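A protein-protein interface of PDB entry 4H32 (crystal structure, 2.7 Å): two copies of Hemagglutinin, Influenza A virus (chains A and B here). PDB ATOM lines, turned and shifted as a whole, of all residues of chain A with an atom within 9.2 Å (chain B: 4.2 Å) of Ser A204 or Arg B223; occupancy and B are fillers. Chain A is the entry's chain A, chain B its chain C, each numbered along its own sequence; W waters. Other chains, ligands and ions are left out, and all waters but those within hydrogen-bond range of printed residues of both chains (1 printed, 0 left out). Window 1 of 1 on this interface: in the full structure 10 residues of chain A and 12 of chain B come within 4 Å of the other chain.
Of the printed residues of chain A, Arg B223 touches Gly A201, Glu A202 and Ser A204. Of chain A, only Gly A201 comes within 4 Å of Ile B217. No residue of chain A comes within 4 Å of Asp B222. No residue of chain A comes within 4 Å of Ile B224. Of the printed residues of chain B, Ile A197 touches Arg B214. Printed residues of chain B within 4 Å of Gly A201: Ile B217 (3.7 Å) and Arg B223 (3.7 Å). Of the printed residues of chain B, Glu A206 touches Arg B214. His B177 touches none of the printed residues of chain A. The nearest printed residue of chain B that does not touch Ser A204 is Gly B94 (5.7 Å). The nearest printed residue of chain A that does not touch Asn B95 is Glu A202 (4.4 Å).
The backbone carbonyl oxygen of Arg A238 lies within hydrogen-bond range of the backbone NH of Asn A199, at 2.7 Å. The side-chain carboxylate (OE2) of Glu A202 lies within salt-bridge range of the side-chain amino group (NZ) of Lys A203 (3.0 Å). N of Asn B95 is in hydrogen-bond range of O of Ile B224, at 3.2 Å. The backbone carbonyl oxygen of Arg B223 sits at hydrogen-bond distance from the backbone NH of Asn B178 (2.8 Å). O of Asp B215 lies within hydrogen-bond range of NH2 of Arg B223 (2.5 Å). The backbone carbonyl oxygen of His B220 lies within hydrogen-bond range of the guanidinium group of Arg B223, at 3.2 Å.
Among the printed residues, merely in contact across the chains: Ile A197 with Arg B214 (3.9 Å), Asn A199 with Arg B214 (3.6 Å), Gly A201 with Ile B217 (3.7 Å), Gly A201 with Arg B223 (3.7 Å), Glu A202 with Pro B93 (3.4 Å), Glu A202 with Gly B94 (3.8 Å), Lys A203 with Asn B95 (3.2 Å) and Ser A204 with Arg B223 (3.99 Å).
Water W1 lies within hydrogen-bond range of OG of Ser A204, OD1 of Asn B95 and O of Glu A202.
Hydrophobic or aromatic side chains of chain A within 4 Å of the printed part of chain B: Ile A197. Among the printed residues, 15 pairs touch across the chains. Among the printed residues, Asp or Glu carboxylates within 4 Å of a Lys or Arg side-chain nitrogen of the other chain: Glu A206 with Arg B214 (3.4 Å) and Arg A238 with Asp B215 (2.7 Å).
No position is printed for both chains. Of the 15 pairs that touch across the chains among the printed residues, none has its exchanged pair printed and touching as well.
OD1 of Asn A199 lies within hydrogen-bond range of N of Asp B215, 2.8 Å away. NH1 of Arg B223 lies within hydrogen-bond range of O of Glu A202 (3.0 Å). The backbone carbonyl oxygen of Gly B94 is in hydrogen-bond range of the side-chain amino group of Lys A203 (3.0 Å). The backbone carbonyl oxygen (O) of Ser A204 is in hydrogen-bond range of the side-chain amide nitrogen (ND2) of Asn B95 (2.8 Å). The side-chain hydroxyl (OG) of Ser A204 lies within hydrogen-bond range of the guanidinium group (NE) of Arg B214. The side-chain carboxylate (OE1) of Glu A206 lies within salt-bridge range of the guanidinium group (NH2) of Arg B214 (3.4 Å). OD2 of Asp B215 is in salt-bridge range of NE of Arg A238 (2.7 Å).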
ATOM      1  N   THR A 196      22.575 -14.249  28.162  1.00  0.00           N
ATOM      2  CA  THR A 196      21.437 -14.060  29.044  1.00  0.00           C
ATOM      3  C   THR A 196      21.099 -12.582  29.028  1.00  0.00           C
ATOM      4  O   THR A 196      21.918 -11.745  29.409  1.00  0.00           O
ATOM      5  CB  THR A 196      21.746 -14.508  30.480  1.00  0.00           C
ATOM      6  OG1 THR A 196      21.864 -15.936  30.518  1.00  0.00           O
ATOM      7  CG2 THR A 196      20.630 -14.072  31.420  1.00  0.00           C
ATOM      8  N   ILE A 197      19.900 -12.258  28.563  1.00  0.00           N
ATOM      9  CA  ILE A 197      19.524 -10.866  28.383  1.00  0.00           C
ATOM     10  C   ILE A 197      18.367 -10.455  29.278  1.00  0.00           C
ATOM     11  O   ILE A 197      17.315 -11.090  29.281  1.00  0.00           O
ATOM     12  CB  ILE A 197      19.170 -10.562  26.915  1.00  0.00           C
ATOM     13  CG1 ILE A 197      20.385 -10.805  26.019  1.00  0.00           C
ATOM     14  CG2 ILE A 197      18.660  -9.129  26.774  1.00  0.00           C
ATOM     15  CD1 ILE A 197      20.117 -10.575  24.547  1.00  0.00           C
ATOM     16  N   PHE A 198      18.585  -9.390  30.043  1.00  0.00           N
ATOM     17  CA  PHE A 198      17.547  -8.802  30.877  1.00  0.00           C
ATOM     18  C   PHE A 198      16.931  -7.614  30.148  1.00  0.00           C
ATOM     19  O   PHE A 198      17.637  -6.690  29.757  1.00  0.00           O
ATOM     20  CB  PHE A 198      18.141  -8.340  32.211  1.00  0.00           C
ATOM     21  CG  PHE A 198      18.251  -9.429  33.245  1.00  0.00           C
ATOM     22  CD1 PHE A 198      17.823  -9.210  34.542  1.00  0.00           C
ATOM     23  CD2 PHE A 198      18.775 -10.670  32.920  1.00  0.00           C
ATOM     24  CE1 PHE A 198      17.918 -10.203  35.495  1.00  0.00           C
ATOM     25  CE2 PHE A 198      18.872 -11.669  33.869  1.00  0.00           C
ATOM     26  CZ  PHE A 198      18.443 -11.436  35.157  1.00  0.00           C
ATOM     27  N   ASN A 199      15.617  -7.633  29.962  1.00  0.00           N
ATOM     28  CA  ASN A 199      14.944  -6.535  29.276  1.00  0.00           C
ATOM     29  C   ASN A 199      14.107  -5.653  30.193  1.00  0.00           C
ATOM     30  O   ASN A 199      13.108  -6.105  30.744  1.00  0.00           O
ATOM     31  CB  ASN A 199      14.039  -7.065  28.162  1.00  0.00           C
ATOM     32  CG  ASN A 199      14.797  -7.837  27.100  1.00  0.00           C
ATOM     33  OD1 ASN A 199      15.331  -7.261  26.152  1.00  0.00           O
ATOM     34  ND2 ASN A 199      14.833  -9.153  27.248  1.00  0.00           N
ATOM     35  N   PHE A 200      14.523  -4.405  30.372  1.00  0.00           N
ATOM     36  CA  PHE A 200      13.679  -3.425  31.040  1.00  0.00           C
ATOM     37  C   PHE A 200      13.212  -2.375  30.035  1.00  0.00           C
ATOM     38  O   PHE A 200      13.769  -1.279  29.959  1.00  0.00           O
ATOM     39  CB  PHE A 200      14.399  -2.769  32.222  1.00  0.00           C
ATOM     40  CG  PHE A 200      13.600  -1.679  32.883  1.00  0.00           C
ATOM     41  CD1 PHE A 200      12.338  -1.941  33.388  1.00  0.00           C
ATOM     42  CD2 PHE A 200      14.106  -0.395  32.989  1.00  0.00           C
ATOM     43  CE1 PHE A 200      11.597  -0.946  33.989  1.00  0.00           C
ATOM     44  CE2 PHE A 200      13.371   0.606  33.591  1.00  0.00           C
ATOM     45  CZ  PHE A 200      12.112   0.330  34.093  1.00  0.00           C
ATOM     46  N   GLY A 201      12.191  -2.726  29.259  1.00  0.00           N
ATOM     47  CA  GLY A 201      11.723  -1.876  28.184  1.00  0.00           C
ATOM     48  C   GLY A 201      12.744  -1.913  27.065  1.00  0.00           C
ATOM     49  O   GLY A 201      13.202  -2.983  26.666  1.00  0.00           O
ATOM     50  N   GLU A 202      13.126  -0.746  26.566  1.00  0.00           N
ATOM     51  CA  GLU A 202      14.124  -0.686  25.508  1.00  0.00           C
ATOM     52  C   GLU A 202      15.524  -0.947  26.065  1.00  0.00           C
ATOM     53  O   GLU A 202      16.455  -1.256  25.316  1.00  0.00           O
ATOM     54  CB  GLU A 202      14.077   0.661  24.788  1.00  0.00           C
ATOM     55  CG  GLU A 202      14.584   1.825  25.618  1.00  0.00           C
ATOM     56  CD  GLU A 202      14.720   3.101  24.805  1.00  0.00           C
ATOM     57  OE1 GLU A 202      14.572   3.035  23.567  1.00  0.00           O
ATOM     58  OE2 GLU A 202      14.976   4.168  25.401  1.00  0.00           O
ATOM     59  N   LYS A 203      15.666  -0.833  27.384  1.00  0.00           N
ATOM     60  CA  LYS A 203      16.963  -1.020  28.033  1.00  0.00           C
ATOM     61  C   LYS A 203      17.293  -2.495  28.209  1.00  0.00           C
ATOM     62  O   LYS A 203      16.415  -3.297  28.514  1.00  0.00           O
ATOM     63  CB  LYS A 203      17.000  -0.322  29.396  1.00  0.00           C
ATOM     64  CG  LYS A 203      16.542   1.128  29.366  1.00  0.00           C
ATOM     65  CD  LYS A 203      17.238   1.903  28.254  1.00  0.00           C
ATOM     66  CE  LYS A 203      16.654   3.288  28.123  1.00  0.00           C
ATOM     67  NZ  LYS A 203      17.440   4.129  27.196  1.00  0.00           N
ATOM     68  N   SER A 204      18.558  -2.857  28.030  1.00  0.00           N
ATOM     69  CA  SER A 204      18.938  -4.256  28.174  1.00  0.00           C
ATOM     70  C   SER A 204      20.360  -4.465  28.682  1.00  0.00           C
ATOM     71  O   SER A 204      21.271  -3.688  28.390  1.00  0.00           O
ATOM     72  CB  SER A 204      18.740  -5.010  26.858  1.00  0.00           C
ATOM     73  OG  SER A 204      19.669  -4.583  25.878  1.00  0.00           O
ATOM     74  N   GLU A 205      20.528  -5.536  29.449  1.00  0.00           N
ATOM     75  CA  GLU A 205      21.836  -5.984  29.890  1.00  0.00           C
ATOM     76  C   GLU A 205      22.042  -7.381  29.344  1.00  0.00           C
ATOM     77  O   GLU A 205      21.134  -8.209  29.392  1.00  0.00           O
ATOM     78  CB  GLU A 205      21.909  -6.046  31.413  1.00  0.00           C
ATOM     79  CG  GLU A 205      21.720  -4.722  32.118  1.00  0.00           C
ATOM     80  CD  GLU A 205      21.852  -4.862  33.622  1.00  0.00           C
ATOM     81  OE1 GLU A 205      22.952  -5.235  34.090  1.00  0.00           O
ATOM     82  OE2 GLU A 205      20.854  -4.614  34.332  1.00  0.00           O
ATOM     83  N   GLU A 206      23.233  -7.647  28.826  1.00  0.00           N
ATOM     84  CA  GLU A 206      23.554  -8.989  28.366  1.00  0.00           C
ATOM     85  C   GLU A 206      24.627  -9.611  29.242  1.00  0.00           C
ATOM     86  O   GLU A 206      25.659  -8.998  29.506  1.00  0.00           O
ATOM     87  CB  GLU A 206      24.001  -8.978  26.904  1.00  0.00           C
ATOM     88  CG  GLU A 206      24.309 -10.356  26.361  1.00  0.00           C
ATOM     89  CD  GLU A 206      24.372 -10.389  24.852  1.00  0.00           C
ATOM     90  OE1 GLU A 206      24.046  -9.367  24.217  1.00  0.00           O
ATOM     91  OE2 GLU A 206      24.745 -11.443  24.300  1.00  0.00           O
ATOM     92  N   PHE A 207      24.374 -10.831  29.699  1.00  0.00           N
ATOM     93  CA  PHE A 207      25.344 -11.550  30.512  1.00  0.00           C
ATOM     94  C   PHE A 207      25.956 -12.714  29.742  1.00  0.00           C
ATOM     95  O   PHE A 207      25.256 -13.470  29.069  1.00  0.00           O
ATOM     96  CB  PHE A 207      24.702 -12.043  31.808  1.00  0.00           C
ATOM     97  CG  PHE A 207      24.173 -10.940  32.680  1.00  0.00           C
ATOM     98  CD1 PHE A 207      24.983 -10.342  33.631  1.00  0.00           C
ATOM     99  CD2 PHE A 207      22.865 -10.499  32.548  1.00  0.00           C
ATOM    100  CE1 PHE A 207      24.502  -9.326  34.435  1.00  0.00           C
ATOM    101  CE2 PHE A 207      22.376  -9.483  33.349  1.00  0.00           C
ATOM    102  CZ  PHE A 207      23.196  -8.896  34.295  1.00  0.00           C
ATOM    103  N   LEU A 237       9.917  -6.869  33.666  1.00  0.00           N
ATOM    104  CA  LEU A 237      11.213  -7.394  33.270  1.00  0.00           C
ATOM    105  C   LEU A 237      11.026  -8.676  32.476  1.00  0.00           C
ATOM    106  O   LEU A 237      10.314  -9.575  32.915  1.00  0.00           O
ATOM    107  CB  LEU A 237      12.072  -7.683  34.502  1.00  0.00           C
ATOM    108  CG  LEU A 237      13.383  -8.422  34.199  1.00  0.00           C
ATOM    109  CD1 LEU A 237      14.348  -7.537  33.421  1.00  0.00           C
ATOM    110  CD2 LEU A 237      14.033  -8.945  35.462  1.00  0.00           C
ATOM    111  N   ARG A 238      11.660  -8.757  31.310  1.00  0.00           N
ATOM    112  CA  ARG A 238      11.634  -9.978  30.510  1.00  0.00           C
ATOM    113  C   ARG A 238      13.040 -10.525  30.295  1.00  0.00           C
ATOM    114  O   ARG A 238      13.940  -9.806  29.868  1.00  0.00           O
ATOM    115  CB  ARG A 238      10.928  -9.745  29.172  1.00  0.00           C
ATOM    116  CG  ARG A 238       9.413  -9.864  29.245  1.00  0.00           C
ATOM    117  CD  ARG A 238       8.759  -9.562  27.910  1.00  0.00           C
ATOM    118  NE  ARG A 238       8.480  -8.138  27.751  1.00  0.00           N
ATOM    119  CZ  ARG A 238       7.290  -7.583  27.957  1.00  0.00           C
ATOM    120  NH1 ARG A 238       6.259  -8.331  28.324  1.00  0.00           N
ATOM    121  NH2 ARG A 238       7.128  -6.277  27.789  1.00  0.00           N
ATOM    122  N   PHE B  92      15.883   5.017  18.141  1.00  0.00           N
ATOM    123  CA  PHE B  92      16.294   3.627  17.974  1.00  0.00           C
ATOM    124  C   PHE B  92      16.581   3.050  19.361  1.00  0.00           C
ATOM    125  O   PHE B  92      17.370   3.613  20.117  1.00  0.00           O
ATOM    126  CB  PHE B  92      17.532   3.523  17.072  1.00  0.00           C
ATOM    127  CG  PHE B  92      17.773   2.142  16.511  1.00  0.00           C
ATOM    128  CD1 PHE B  92      17.524   1.871  15.173  1.00  0.00           C
ATOM    129  CD2 PHE B  92      18.255   1.121  17.315  1.00  0.00           C
ATOM    130  CE1 PHE B  92      17.744   0.606  14.649  1.00  0.00           C
ATOM    131  CE2 PHE B  92      18.477  -0.147  16.798  1.00  0.00           C
ATOM    132  CZ  PHE B  92      18.220  -0.404  15.462  1.00  0.00           C
ATOM    133  N   PRO B  93      15.934   1.922  19.695  1.00  0.00           N
ATOM    134  CA  PRO B  93      16.017   1.337  21.037  1.00  0.00           C
ATOM    135  C   PRO B  93      17.444   0.982  21.448  1.00  0.00           C
ATOM    136  O   PRO B  93      18.228   0.503  20.628  1.00  0.00           O
ATOM    137  CB  PRO B  93      15.181   0.060  20.915  1.00  0.00           C
ATOM    138  CG  PRO B  93      14.280   0.298  19.758  1.00  0.00           C
ATOM    139  CD  PRO B  93      15.085   1.122  18.799  1.00  0.00           C
ATOM    140  N   GLY B  94      17.766   1.217  22.716  1.00  0.00           N
ATOM    141  CA  GLY B  94      19.073   0.883  23.246  1.00  0.00           C
ATOM    142  C   GLY B  94      19.395   1.585  24.549  1.00  0.00           C
ATOM    143  O   GLY B  94      18.519   2.164  25.189  1.00  0.00           O
ATOM    144  N   ASN B  95      20.664   1.526  24.940  1.00  0.00           N
ATOM    145  CA  ASN B  95      21.128   2.146  26.174  1.00  0.00           C
ATOM    146  C   ASN B  95      21.989   3.362  25.883  1.00  0.00           C
ATOM    147  O   ASN B  95      22.770   3.365  24.935  1.00  0.00           O
ATOM    148  CB  ASN B  95      21.949   1.150  27.000  1.00  0.00           C
ATOM    149  CG  ASN B  95      21.228  -0.168  27.221  1.00  0.00           C
ATOM    150  OD1 ASN B  95      20.043  -0.193  27.550  1.00  0.00           O
ATOM    151  ND2 ASN B  95      21.942  -1.272  27.036  1.00  0.00           N
ATOM    152  N   ILE B 176      27.133   1.834  19.069  1.00  0.00           N
ATOM    153  CA  ILE B 176      27.582   0.517  18.660  1.00  0.00           C
ATOM    154  C   ILE B 176      26.340  -0.331  18.425  1.00  0.00           C
ATOM    155  O   ILE B 176      25.439  -0.367  19.266  1.00  0.00           O
ATOM    156  CB  ILE B 176      28.462  -0.140  19.728  1.00  0.00           C
ATOM    157  CG1 ILE B 176      29.702   0.715  19.987  1.00  0.00           C
ATOM    158  CG2 ILE B 176      28.847  -1.555  19.303  1.00  0.00           C
ATOM    159  CD1 ILE B 176      30.609   0.840  18.789  1.00  0.00           C
ATOM    160  N   HIS B 177      26.288  -0.993  17.274  1.00  0.00           N
ATOM    161  CA  HIS B 177      25.114  -1.759  16.896  1.00  0.00           C
ATOM    162  C   HIS B 177      25.157  -3.157  17.485  1.00  0.00           C
ATOM    163  O   HIS B 177      26.007  -3.965  17.119  1.00  0.00           O
ATOM    164  CB  HIS B 177      24.981  -1.839  15.376  1.00  0.00           C
ATOM    165  CG  HIS B 177      23.736  -2.538  14.920  1.00  0.00           C
ATOM    166  ND1 HIS B 177      23.651  -3.197  13.714  1.00  0.00           N
ATOM    167  CD2 HIS B 177      22.523  -2.676  15.511  1.00  0.00           C
ATOM    168  CE1 HIS B 177      22.437  -3.712  13.580  1.00  0.00           C
ATOM    169  NE2 HIS B 177      21.737  -3.408  14.654  1.00  0.00           N
ATOM    170  N   ASN B 178      24.242  -3.432  18.408  1.00  0.00           N
ATOM    171  CA  ASN B 178      24.115  -4.766  18.981  1.00  0.00           C
ATOM    172  C   ASN B 178      23.146  -5.632  18.168  1.00  0.00           C
ATOM    173  O   ASN B 178      21.928  -5.569  18.351  1.00  0.00           O
ATOM    174  CB  ASN B 178      23.682  -4.687  20.446  1.00  0.00           C
ATOM    175  CG  ASN B 178      24.747  -4.062  21.337  1.00  0.00           C
ATOM    176  OD1 ASN B 178      25.945  -4.189  21.076  1.00  0.00           O
ATOM    177  ND2 ASN B 178      24.315  -3.390  22.397  1.00  0.00           N
ATOM    178  N   ARG B 214      17.076  -9.282  21.942  1.00  0.00           N
ATOM    179  CA  ARG B 214      16.374  -8.514  22.967  1.00  0.00           C
ATOM    180  C   ARG B 214      14.872  -8.661  22.781  1.00  0.00           C
ATOM    181  O   ARG B 214      14.412  -9.070  21.716  1.00  0.00           O
ATOM    182  CB  ARG B 214      16.744  -7.030  22.900  1.00  0.00           C
ATOM    183  CG  ARG B 214      17.979  -6.647  23.693  1.00  0.00           C
ATOM    184  CD  ARG B 214      19.250  -7.103  23.006  1.00  0.00           C
ATOM    185  NE  ARG B 214      20.441  -6.550  23.641  1.00  0.00           N
ATOM    186  CZ  ARG B 214      21.681  -6.758  23.210  1.00  0.00           C
ATOM    187  NH1 ARG B 214      21.894  -7.509  22.137  1.00  0.00           N
ATOM    188  NH2 ARG B 214      22.707  -6.214  23.850  1.00  0.00           N
ATOM    189  N   ASP B 215      14.109  -8.329  23.818  1.00  0.00           N
ATOM    190  CA  ASP B 215      12.656  -8.310  23.707  1.00  0.00           C
ATOM    191  C   ASP B 215      12.279  -7.310  22.617  1.00  0.00           C
ATOM    192  O   ASP B 215      12.856  -6.227  22.539  1.00  0.00           O
ATOM    193  CB  ASP B 215      12.022  -7.913  25.040  1.00  0.00           C
ATOM    194  CG  ASP B 215      10.542  -8.236  25.103  1.00  0.00           C
ATOM    195  OD1 ASP B 215      10.160  -9.365  24.724  1.00  0.00           O
ATOM    196  OD2 ASP B 215       9.760  -7.356  25.523  1.00  0.00           O
ATOM    197  N   ILE B 217      11.003  -4.415  20.686  1.00  0.00           N
ATOM    198  CA  ILE B 217      10.474  -3.076  20.889  1.00  0.00           C
ATOM    199  C   ILE B 217      10.601  -2.323  19.571  1.00  0.00           C
ATOM    200  O   ILE B 217      11.660  -2.351  18.938  1.00  0.00           O
ATOM    201  CB  ILE B 217      11.239  -2.321  22.018  1.00  0.00           C
ATOM    202  CG1 ILE B 217      10.579  -2.561  23.382  1.00  0.00           C
ATOM    203  CG2 ILE B 217      11.302  -0.824  21.731  1.00  0.00           C
ATOM    204  CD1 ILE B 217      10.852  -3.927  23.977  1.00  0.00           C
ATOM    205  N   HIS B 220      12.044  -4.064  16.738  1.00  0.00           N
ATOM    206  CA  HIS B 220      13.477  -4.324  16.788  1.00  0.00           C
ATOM    207  C   HIS B 220      13.821  -5.286  17.912  1.00  0.00           C
ATOM    208  O   HIS B 220      13.424  -5.078  19.058  1.00  0.00           O
ATOM    209  CB  HIS B 220      14.260  -3.027  16.994  1.00  0.00           C
ATOM    210  CG  HIS B 220      14.430  -2.217  15.749  1.00  0.00           C
ATOM    211  ND1 HIS B 220      15.410  -2.473  14.817  1.00  0.00           N
ATOM    212  CD2 HIS B 220      13.745  -1.142  15.288  1.00  0.00           C
ATOM    213  CE1 HIS B 220      15.324  -1.603  13.835  1.00  0.00           C
ATOM    214  NE2 HIS B 220      14.321  -0.779  14.091  1.00  0.00           N
ATOM    215  N   ASP B 222      17.111  -6.022  17.975  1.00  0.00           N
ATOM    216  CA  ASP B 222      18.475  -5.546  18.135  1.00  0.00           C
ATOM    217  C   ASP B 222      18.476  -4.209  18.870  1.00  0.00           C
ATOM    218  O   ASP B 222      17.432  -3.581  19.038  1.00  0.00           O
ATOM    219  CB  ASP B 222      19.170  -5.432  16.777  1.00  0.00           C
ATOM    220  CG  ASP B 222      18.378  -4.612  15.777  1.00  0.00           C
ATOM    221  OD1 ASP B 222      18.992  -4.081  14.830  1.00  0.00           O
ATOM    222  OD2 ASP B 222      17.145  -4.494  15.933  1.00  0.00           O
ATOM    223  N   ARG B 223      19.649  -3.780  19.318  1.00  0.00           N
ATOM    224  CA  ARG B 223      19.762  -2.547  20.082  1.00  0.00           C
ATOM    225  C   ARG B 223      20.962  -1.720  19.634  1.00  0.00           C
ATOM    226  O   ARG B 223      21.795  -2.180  18.851  1.00  0.00           O
ATOM    227  CB  ARG B 223      19.876  -2.859  21.580  1.00  0.00           C
ATOM    228  CG  ARG B 223      18.632  -3.495  22.182  1.00  0.00           C
ATOM    229  CD  ARG B 223      17.471  -2.516  22.197  1.00  0.00           C
ATOM    230  NE  ARG B 223      16.219  -3.123  21.747  1.00  0.00           N
ATOM    231  CZ  ARG B 223      15.333  -3.703  22.550  1.00  0.00           C
ATOM    232  NH1 ARG B 223      15.555  -3.767  23.855  1.00  0.00           N
ATOM    233  NH2 ARG B 223      14.222  -4.220  22.048  1.00  0.00           N
ATOM    234  N   ILE B 224      21.028  -0.488  20.128  1.00  0.00           N
ATOM    235  CA  ILE B 224      22.207   0.351  19.960  1.00  0.00           C
ATOM    236  C   ILE B 224      22.654   0.913  21.302  1.00  0.00           C
ATOM    237  O   ILE B 224      21.881   1.555  22.007  1.00  0.00           O
ATOM    238  CB  ILE B 224      21.958   1.531  18.999  1.00  0.00           C
ATOM    239  CG1 ILE B 224      21.865   1.040  17.558  1.00  0.00           C
ATOM    240  CG2 ILE B 224      23.085   2.551  19.105  1.00  0.00           C
ATOM    241  CD1 ILE B 224      21.669   2.164  16.565  1.00  0.00           C
HETATM  242  O   HOH W   1      19.457  -2.007  25.281  1.00  0.00           O
